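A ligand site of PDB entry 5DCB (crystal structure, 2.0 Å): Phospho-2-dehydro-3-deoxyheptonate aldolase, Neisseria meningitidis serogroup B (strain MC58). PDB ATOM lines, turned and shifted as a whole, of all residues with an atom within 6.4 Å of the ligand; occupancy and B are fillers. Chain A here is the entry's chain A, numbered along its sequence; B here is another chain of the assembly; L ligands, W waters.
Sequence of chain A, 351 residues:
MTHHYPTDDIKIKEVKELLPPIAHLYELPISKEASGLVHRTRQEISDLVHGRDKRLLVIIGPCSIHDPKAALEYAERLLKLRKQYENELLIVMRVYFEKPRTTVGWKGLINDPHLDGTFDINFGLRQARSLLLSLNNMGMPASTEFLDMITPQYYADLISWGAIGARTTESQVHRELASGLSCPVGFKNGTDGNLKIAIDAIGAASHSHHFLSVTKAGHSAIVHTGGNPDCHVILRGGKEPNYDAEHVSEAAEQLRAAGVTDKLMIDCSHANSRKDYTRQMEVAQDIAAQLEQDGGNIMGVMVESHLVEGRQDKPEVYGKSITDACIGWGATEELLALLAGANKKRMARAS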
ATOM      1  N   ARG A  42      12.151  36.466  -7.829  1.00  0.00           N
ATOM      2  CA  ARG A  42      10.825  35.865  -7.867  1.00  0.00           C
ATOM      3  C   ARG A  42       9.738  36.908  -8.080  1.00  0.00           C
ATOM      4  O   ARG A  42       8.850  36.691  -8.885  1.00  0.00           O
ATOM      5  CB  ARG A  42      10.542  35.081  -6.585  1.00  0.00           C
ATOM      6  CG  ARG A  42      11.376  33.830  -6.410  1.00  0.00           C
ATOM      7  CD  ARG A  42      11.192  33.272  -5.003  1.00  0.00           C
ATOM      8  NE  ARG A  42      11.799  31.954  -4.863  1.00  0.00           N
ATOM      9  CZ  ARG A  42      12.023  31.338  -3.711  1.00  0.00           C
ATOM     10  NH1 ARG A  42      11.737  31.908  -2.547  1.00  0.00           N
ATOM     11  NH2 ARG A  42      12.589  30.152  -3.715  1.00  0.00           N
ATOM     12  N   PHE A 146      12.106  20.587 -11.194  1.00  0.00           N
ATOM     13  CA  PHE A 146      11.936  19.684 -10.086  1.00  0.00           C
ATOM     14  C   PHE A 146      11.322  18.402 -10.588  1.00  0.00           C
ATOM     15  O   PHE A 146      10.230  18.412 -11.145  1.00  0.00           O
ATOM     16  CB  PHE A 146      11.083  20.313  -8.997  1.00  0.00           C
ATOM     17  CG  PHE A 146      11.707  21.521  -8.378  1.00  0.00           C
ATOM     18  CD1 PHE A 146      12.786  21.384  -7.525  1.00  0.00           C
ATOM     19  CD2 PHE A 146      11.248  22.783  -8.678  1.00  0.00           C
ATOM     20  CE1 PHE A 146      13.372  22.493  -6.940  1.00  0.00           C
ATOM     21  CE2 PHE A 146      11.835  23.888  -8.102  1.00  0.00           C
ATOM     22  CZ  PHE A 146      12.895  23.745  -7.239  1.00  0.00           C
ATOM     23  N   MET A 149       9.254  15.186  -5.480  1.00  0.00           N
ATOM     24  CA  MET A 149       8.661  15.943  -4.396  1.00  0.00           C
ATOM     25  C   MET A 149       9.525  16.108  -3.153  1.00  0.00           C
ATOM     26  O   MET A 149       9.120  16.820  -2.226  1.00  0.00           O
ATOM     27  CB  MET A 149       7.298  15.314  -4.006  1.00  0.00           C
ATOM     28  CG  MET A 149       6.153  15.761  -4.912  1.00  0.00           C
ATOM     29  SD  MET A 149       6.356  15.558  -6.719  1.00  0.00           S
ATOM     30  CE  MET A 149       6.489  13.774  -6.827  1.00  0.00           C
ATOM     31  N   ILE A 150      10.707  15.488  -3.150  1.00  0.00           N
ATOM     32  CA  ILE A 150      11.620  15.492  -1.989  1.00  0.00           C
ATOM     33  C   ILE A 150      12.827  16.425  -2.208  1.00  0.00           C
ATOM     34  O   ILE A 150      13.178  17.165  -1.293  1.00  0.00           O
ATOM     35  CB  ILE A 150      12.062  14.074  -1.633  1.00  0.00           C
ATOM     36  CG1 ILE A 150      10.887  13.300  -1.037  1.00  0.00           C
ATOM     37  CG2 ILE A 150      13.229  14.060  -0.650  1.00  0.00           C
ATOM     38  CD1 ILE A 150      11.117  11.811  -1.003  1.00  0.00           C
ATOM     39  N   PRO A 152      13.060  19.247  -3.594  1.00  0.00           N
ATOM     40  CA  PRO A 152      12.936  20.685  -3.341  1.00  0.00           C
ATOM     41  C   PRO A 152      13.254  21.098  -1.906  1.00  0.00           C
ATOM     42  O   PRO A 152      13.769  22.186  -1.672  1.00  0.00           O
ATOM     43  CB  PRO A 152      11.483  20.998  -3.728  1.00  0.00           C
ATOM     44  CG  PRO A 152      11.101  19.889  -4.680  1.00  0.00           C
ATOM     45  CD  PRO A 152      11.843  18.682  -4.202  1.00  0.00           C
ATOM     46  N   GLN A 153      13.019  20.222  -0.950  1.00  0.00           N
ATOM     47  CA  GLN A 153      13.350  20.523   0.443  1.00  0.00           C
ATOM     48  C   GLN A 153      14.836  20.773   0.674  1.00  0.00           C
ATOM     49  O   GLN A 153      15.200  21.370   1.689  1.00  0.00           O
ATOM     50  CB  GLN A 153      12.847  19.403   1.350  1.00  0.00           C
ATOM     51  CG  GLN A 153      11.350  19.347   1.487  1.00  0.00           C
ATOM     52  CD  GLN A 153      10.822  20.516   2.295  1.00  0.00           C
ATOM     53  OE1 GLN A 153      10.995  21.671   1.893  1.00  0.00           O
ATOM     54  NE2 GLN A 153      10.180  20.222   3.437  1.00  0.00           N
ATOM     55  N   ALA A 156      15.187  24.276  -2.774  1.00  0.00           N
ATOM     56  CA  ALA A 156      14.226  25.202  -3.431  1.00  0.00           C
ATOM     57  C   ALA A 156      14.311  26.646  -2.939  1.00  0.00           C
ATOM     58  O   ALA A 156      13.919  27.562  -3.681  1.00  0.00           O
ATOM     59  CB  ALA A 156      12.797  24.719  -3.336  1.00  0.00           C
ATOM     60  N   ASP A 157      14.815  26.845  -1.727  1.00  0.00           N
ATOM     61  CA  ASP A 157      15.015  28.162  -1.168  1.00  0.00           C
ATOM     62  C   ASP A 157      16.002  29.000  -1.982  1.00  0.00           C
ATOM     63  O   ASP A 157      16.001  30.240  -1.872  1.00  0.00           O
ATOM     64  CB  ASP A 157      15.459  28.089   0.323  1.00  0.00           C
ATOM     65  CG  ASP A 157      16.764  27.361   0.529  1.00  0.00           C
ATOM     66  OD1 ASP A 157      16.923  26.222   0.005  1.00  0.00           O
ATOM     67  OD2 ASP A 157      17.667  27.922   1.182  1.00  0.00           O
ATOM     68  N   LEU A 177       2.907  19.622  -6.189  1.00  0.00           N
ATOM     69  CA  LEU A 177       4.190  20.235  -5.871  1.00  0.00           C
ATOM     70  C   LEU A 177       4.266  21.696  -6.320  1.00  0.00           C
ATOM     71  O   LEU A 177       4.585  22.596  -5.526  1.00  0.00           O
ATOM     72  CB  LEU A 177       5.368  19.436  -6.472  1.00  0.00           C
ATOM     73  CG  LEU A 177       6.703  20.133  -6.296  1.00  0.00           C
ATOM     74  CD1 LEU A 177       7.054  20.233  -4.801  1.00  0.00           C
ATOM     75  CD2 LEU A 177       7.787  19.372  -7.047  1.00  0.00           C
ATOM     76  N   GLY A 180       2.861  24.582  -4.344  1.00  0.00           N
ATOM     77  CA  GLY A 180       3.546  24.932  -3.104  1.00  0.00           C
ATOM     78  C   GLY A 180       4.984  25.412  -3.295  1.00  0.00           C
ATOM     79  O   GLY A 180       5.693  25.637  -2.318  1.00  0.00           O
ATOM     80  N   LEU A 181       5.430  25.578  -4.529  1.00  0.00           N
ATOM     81  CA  LEU A 181       6.826  26.008  -4.751  1.00  0.00           C
ATOM     82  C   LEU A 181       6.898  27.499  -4.561  1.00  0.00           C
ATOM     83  O   LEU A 181       6.027  28.247  -5.048  1.00  0.00           O
ATOM     84  CB  LEU A 181       7.337  25.617  -6.141  1.00  0.00           C
ATOM     85  CG  LEU A 181       7.683  24.133  -6.306  1.00  0.00           C
ATOM     86  CD1 LEU A 181       8.011  23.785  -7.732  1.00  0.00           C
ATOM     87  CD2 LEU A 181       8.861  23.751  -5.408  1.00  0.00           C
ATOM     88  N   SER A 182       7.946  27.920  -3.851  1.00  0.00           N
ATOM     89  CA  SER A 182       8.173  29.341  -3.522  1.00  0.00           C
ATOM     90  C   SER A 182       8.440  30.203  -4.749  1.00  0.00           C
ATOM     91  O   SER A 182       8.160  31.385  -4.750  1.00  0.00           O
ATOM     92  CB  SER A 182       9.275  29.495  -2.473  1.00  0.00           C
ATOM     93  OG  SER A 182       8.877  28.857  -1.245  1.00  0.00           O
ATOM     94  N   CYS A 183       8.942  29.598  -5.799  1.00  0.00           N
ATOM     95  CA  CYS A 183       9.271  30.300  -7.020  1.00  0.00           C
ATOM     96  C   CYS A 183       8.116  30.272  -8.028  1.00  0.00           C
ATOM     97  O   CYS A 183       7.230  29.432  -7.932  1.00  0.00           O
ATOM     98  CB  CYS A 183      10.511  29.658  -7.649  1.00  0.00           C
ATOM     99  SG  CYS A 183      10.322  27.913  -7.978  1.00  0.00           S
ATOM    100  N   PHE A 211       0.264  17.107  -0.634  1.00  0.00           N
ATOM    101  CA  PHE A 211       1.056  16.034  -1.206  1.00  0.00           C
ATOM    102  C   PHE A 211       2.061  15.603  -0.156  1.00  0.00           C
ATOM    103  O   PHE A 211       2.280  16.301   0.849  1.00  0.00           O
ATOM    104  CB  PHE A 211       1.771  16.455  -2.504  1.00  0.00           C
ATOM    105  CG  PHE A 211       2.847  17.490  -2.306  1.00  0.00           C
ATOM    106  CD1 PHE A 211       2.546  18.833  -2.383  1.00  0.00           C
ATOM    107  CD2 PHE A 211       4.167  17.117  -2.071  1.00  0.00           C
ATOM    108  CE1 PHE A 211       3.534  19.797  -2.205  1.00  0.00           C
ATOM    109  CE2 PHE A 211       5.146  18.077  -1.893  1.00  0.00           C
ATOM    110  CZ  PHE A 211       4.837  19.414  -1.947  1.00  0.00           C
ATOM    111  N   LEU A 212       2.642  14.438  -0.393  1.00  0.00           N
ATOM    112  CA  LEU A 212       3.503  13.828   0.603  1.00  0.00           C
ATOM    113  C   LEU A 212       4.959  14.119   0.305  1.00  0.00           C
ATOM    114  O   LEU A 212       5.368  14.106  -0.846  1.00  0.00           O
ATOM    115  CB  LEU A 212       3.269  12.339   0.657  1.00  0.00           C
ATOM    116  CG  LEU A 212       1.841  11.869   0.963  1.00  0.00           C
ATOM    117  CD1 LEU A 212       1.866  10.403   1.312  1.00  0.00           C
ATOM    118  CD2 LEU A 212       1.255  12.660   2.134  1.00  0.00           C
ATOM    119  N   SER A 213       5.743  14.378   1.346  1.00  0.00           N
ATOM    120  CA  SER A 213       7.138  14.708   1.174  1.00  0.00           C
ATOM    121  C   SER A 213       7.830  14.455   2.493  1.00  0.00           C
ATOM    122  O   SER A 213       7.431  13.575   3.239  1.00  0.00           O
ATOM    123  CB  SER A 213       7.289  16.155   0.711  1.00  0.00           C
ATOM    124  OG  SER A 213       8.626  16.450   0.325  1.00  0.00           O
ATOM    125  N   VAL A 214       8.889  15.210   2.773  1.00  0.00           N
ATOM    126  CA  VAL A 214       9.550  15.142   4.049  1.00  0.00           C
ATOM    127  C   VAL A 214       9.692  16.528   4.637  1.00  0.00           C
ATOM    128  O   VAL A 214       9.690  17.522   3.921  1.00  0.00           O
ATOM    129  CB  VAL A 214      10.913  14.435   3.997  1.00  0.00           C
ATOM    130  CG1 VAL A 214      10.755  13.023   3.502  1.00  0.00           C
ATOM    131  CG2 VAL A 214      11.914  15.178   3.123  1.00  0.00           C
ATOM    132  N   LYS A 216      11.899  19.341   6.925  1.00  0.00           N
ATOM    133  CA  LYS A 216      13.312  19.708   6.862  1.00  0.00           C
ATOM    134  C   LYS A 216      14.155  18.737   7.668  1.00  0.00           C
ATOM    135  O   LYS A 216      15.312  18.526   7.337  1.00  0.00           O
ATOM    136  CB  LYS A 216      13.548  21.164   7.309  1.00  0.00           C
ATOM    137  CG  LYS A 216      12.885  22.193   6.392  1.00  0.00           C
ATOM    138  CD  LYS A 216      13.311  22.000   4.944  1.00  0.00           C
ATOM    139  CE  LYS A 216      13.117  23.238   4.080  1.00  0.00           C
ATOM    140  NZ  LYS A 216      11.684  23.593   3.887  1.00  0.00           N
ATOM    141  N   VAL A 223       2.219  17.771   3.073  1.00  0.00           N
ATOM    142  CA  VAL A 223       2.426  19.169   2.780  1.00  0.00           C
ATOM    143  C   VAL A 223       1.117  19.802   2.327  1.00  0.00           C
ATOM    144  O   VAL A 223       0.450  19.294   1.434  1.00  0.00           O
ATOM    145  CB  VAL A 223       3.484  19.366   1.680  1.00  0.00           C
ATOM    146  CG1 VAL A 223       3.704  20.844   1.412  1.00  0.00           C
ATOM    147  CG2 VAL A 223       4.784  18.678   2.054  1.00  0.00           C
ATOM    148  N   THR B   7      12.769  33.034   1.901  1.00  0.00           N
ATOM    149  CA  THR B   7      12.785  32.324   0.625  1.00  0.00           C
ATOM    150  C   THR B   7      12.205  30.909   0.689  1.00  0.00           C
ATOM    151  O   THR B   7      12.034  30.249  -0.345  1.00  0.00           O
ATOM    152  CB  THR B   7      14.218  32.235   0.023  1.00  0.00           C
ATOM    153  OG1 THR B   7      15.071  31.527   0.926  1.00  0.00           O
ATOM    154  CG2 THR B   7      14.785  33.618  -0.226  1.00  0.00           C
ATOM    155  N   ASP B   8      11.899  30.459   1.893  1.00  0.00           N
ATOM    156  CA  ASP B   8      11.556  29.059   2.132  1.00  0.00           C
ATOM    157  C   ASP B   8      10.083  28.908   2.483  1.00  0.00           C
ATOM    158  O   ASP B   8       9.579  29.631   3.314  1.00  0.00           O
ATOM    159  CB  ASP B   8      12.455  28.536   3.265  1.00  0.00           C
ATOM    160  CG  ASP B   8      12.146  27.123   3.645  1.00  0.00           C
ATOM    161  OD1 ASP B   8      11.965  26.278   2.755  1.00  0.00           O
ATOM    162  OD2 ASP B   8      12.082  26.857   4.852  1.00  0.00           O
ATOM    163  N   ASP B   9       9.410  27.960   1.843  1.00  0.00           N
ATOM    164  CA  ASP B   9       8.026  27.623   2.194  1.00  0.00           C
ATOM    165  C   ASP B   9       7.083  28.829   2.104  1.00  0.00           C
ATOM    166  O   ASP B   9       6.126  28.930   2.880  1.00  0.00           O
ATOM    167  CB  ASP B   9       7.950  27.011   3.597  1.00  0.00           C
ATOM    168  CG  ASP B   9       8.448  25.572   3.635  1.00  0.00           C
ATOM    169  OD1 ASP B   9       8.912  25.020   2.613  1.00  0.00           O
ATOM    170  OD2 ASP B   9       8.355  24.971   4.716  1.00  0.00           O
ATOM    171  N   ILE B  10       7.339  29.729   1.175  1.00  0.00           N
ATOM    172  CA  ILE B  10       6.537  30.923   1.027  1.00  0.00           C
ATOM    173  C   ILE B  10       5.066  30.620   0.743  1.00  0.00           C
ATOM    174  O   ILE B  10       4.214  31.350   1.187  1.00  0.00           O
ATOM    175  CB  ILE B  10       7.057  31.847  -0.105  1.00  0.00           C
ATOM    176  CG1 ILE B  10       8.536  32.234   0.083  1.00  0.00           C
ATOM    177  CG2 ILE B  10       6.215  33.120  -0.171  1.00  0.00           C
ATOM    178  CD1 ILE B  10       8.843  32.998   1.360  1.00  0.00           C
ATOM    179  N   LYS B  11       4.775  29.544  -0.011  1.00  0.00           N
ATOM    180  CA  LYS B  11       3.425  29.239  -0.437  1.00  0.00           C
ATOM    181  C   LYS B  11       2.956  27.930   0.191  1.00  0.00           C
ATOM    182  O   LYS B  11       2.129  27.234  -0.366  1.00  0.00           O
ATOM    183  CB  LYS B  11       3.357  29.159  -1.957  1.00  0.00           C
ATOM    184  CG  LYS B  11       3.768  30.466  -2.626  1.00  0.00           C
ATOM    185  CD  LYS B  11       3.824  30.345  -4.142  1.00  0.00           C
ATOM    186  CE  LYS B  11       4.583  31.515  -4.775  1.00  0.00           C
ATOM    187  NZ  LYS B  11       5.183  31.092  -6.073  1.00  0.00           N
ATOM    188  N   ILE B  12       3.467  27.648   1.371  1.00  0.00           N
ATOM    189  CA  ILE B  12       3.104  26.490   2.143  1.00  0.00           C
ATOM    190  C   ILE B  12       2.307  26.937   3.355  1.00  0.00           C
ATOM    191  O   ILE B  12       2.736  27.818   4.087  1.00  0.00           O
ATOM    192  CB  ILE B  12       4.348  25.768   2.640  1.00  0.00           C
ATOM    193  CG1 ILE B  12       5.171  25.294   1.443  1.00  0.00           C
ATOM    194  CG2 ILE B  12       3.996  24.600   3.558  1.00  0.00           C
ATOM    195  CD1 ILE B  12       4.464  24.269   0.577  1.00  0.00           C
ATOM    196  N   VAL B  15       3.322  22.059   6.985  1.00  0.00           N
ATOM    197  CA  VAL B  15       3.955  20.779   6.812  1.00  0.00           C
ATOM    198  C   VAL B  15       3.807  20.063   8.155  1.00  0.00           C
ATOM    199  O   VAL B  15       4.222  20.606   9.156  1.00  0.00           O
ATOM    200  CB  VAL B  15       5.453  20.970   6.515  1.00  0.00           C
ATOM    201  CG1 VAL B  15       6.104  19.626   6.185  1.00  0.00           C
ATOM    202  CG2 VAL B  15       5.630  21.965   5.384  1.00  0.00           C
HETATM  203  N1  LIG L   1      10.339  24.138   0.481  1.00  0.00           N
HETATM  204  C1  LIG L   1       9.770  24.286  -0.863  1.00  0.00           C
HETATM  205  C2  LIG L   1       9.832  25.708  -1.353  1.00  0.00           C
HETATM  206  O1  LIG L   1       9.597  25.940  -2.544  1.00  0.00           O
HETATM  207  C3  LIG L   1       8.310  23.813  -0.864  1.00  0.00           C
HETATM  208  C4  LIG L   1       8.181  22.381  -0.501  1.00  0.00           C
HETATM  209  C5  LIG L   1       8.442  21.406  -1.450  1.00  0.00           C
HETATM  210  C6  LIG L   1       7.872  22.005   0.783  1.00  0.00           C
HETATM  211  C7  LIG L   1       8.362  20.072  -1.116  1.00  0.00           C
HETATM  212  C8  LIG L   1       7.792  20.650   1.125  1.00  0.00           C
HETATM  213  C9  LIG L   1       8.038  19.703   0.174  1.00  0.00           C
HETATM  214  O2  LIG L   1      10.085  26.602  -0.547  1.00  0.00           O
HETATM  215  O   HOH W   1      13.089  24.879   0.565  1.00  0.00           O
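Water W1 lies within hydrogen-bond range of the side-chain carboxylate (OD1) of Asp 8 of chain B (2.8 Å), a nitrogen (N1) of the ligand (2.8 Å) and the backbone NH (N) of Asp 157 (3.5 Å).
Residues that only touch the ligand: Ser 213 (3.3 Å), Gly 180 (3.5 Å), Ala 156 (3.5 Å), Met 149 (3.5 Å), Leu 181 (3.5 Å), Phe 211 (3.7 Å), Lys 216 (3.7 Å), Val 223 (3.7 Å), Leu 177 (3.8 Å) and Pro 152 (3.8 Å). 14 residues have an atom within 4 Å of the ligand: Met 149, Pro 152, Gln 153, Ala 156, Leu 177, Gly 180, Leu 181, Ser 182, Phe 211, Ser 213, Lys 216, Val 223, Asp 8 of chain B and Asp 9 of chain B. The nearest printed residue that does not touch the ligand is Ile 12 of chain B (4.1 Å).
OD1 of Asp 9 of chain B is in salt-bridge range of N1 of the ligand (2.7 Å). A nitrogen (N1) of the ligand lies within salt-bridge range of the side-chain carboxylate (OD1) of Asp 8 of chain B, 3.5 Å away. OE1 of Gln 153 is in hydrogen-bond range of N1 of the ligand, at 2.9 Å. An oxygen (O2) of the ligand sits at hydrogen-bond distance from the backbone NH (N) of Asp 9 of chain B, at 2.8 Å. OG of Ser 182 sits at hydrogen-bond distance from O2 of the ligand, 2.7 Å away. An oxygen (O1) of the ligand is in hydrogen-bond range of the backbone NH of Ser 182 (2.9 Å).
The side-chain hydroxyl (OG) of Ser 182 is in hydrogen-bond range of the backbone NH (N) of Ile 10 of chain B (3.0 Å). OD1 of Asp 9 of chain B lies within salt-bridge range of NZ of Lys 216. O of Leu 181 is in hydrogen-bond range of NZ of Lys 11 of chain B. The side-chain amide nitrogen (NE2) of Gln 153 lies within hydrogen-bond range of the backbone carbonyl oxygen (O) of Val 214. The backbone carbonyl oxygen of Ser 182 lies within hydrogen-bond range of the side-chain amino group of Lys 11 of chain B (3.3 Å). The side-chain carboxylate of Asp 8 of chain B is in salt-bridge range of the side-chain amino group of Lys 216 (2.9 Å). O of Phe 211 lies within hydrogen-bond range of N of Val 223. OG of Ser 182 is in hydrogen-bond range of N of Asp 9 of chain B (3.3 Å).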
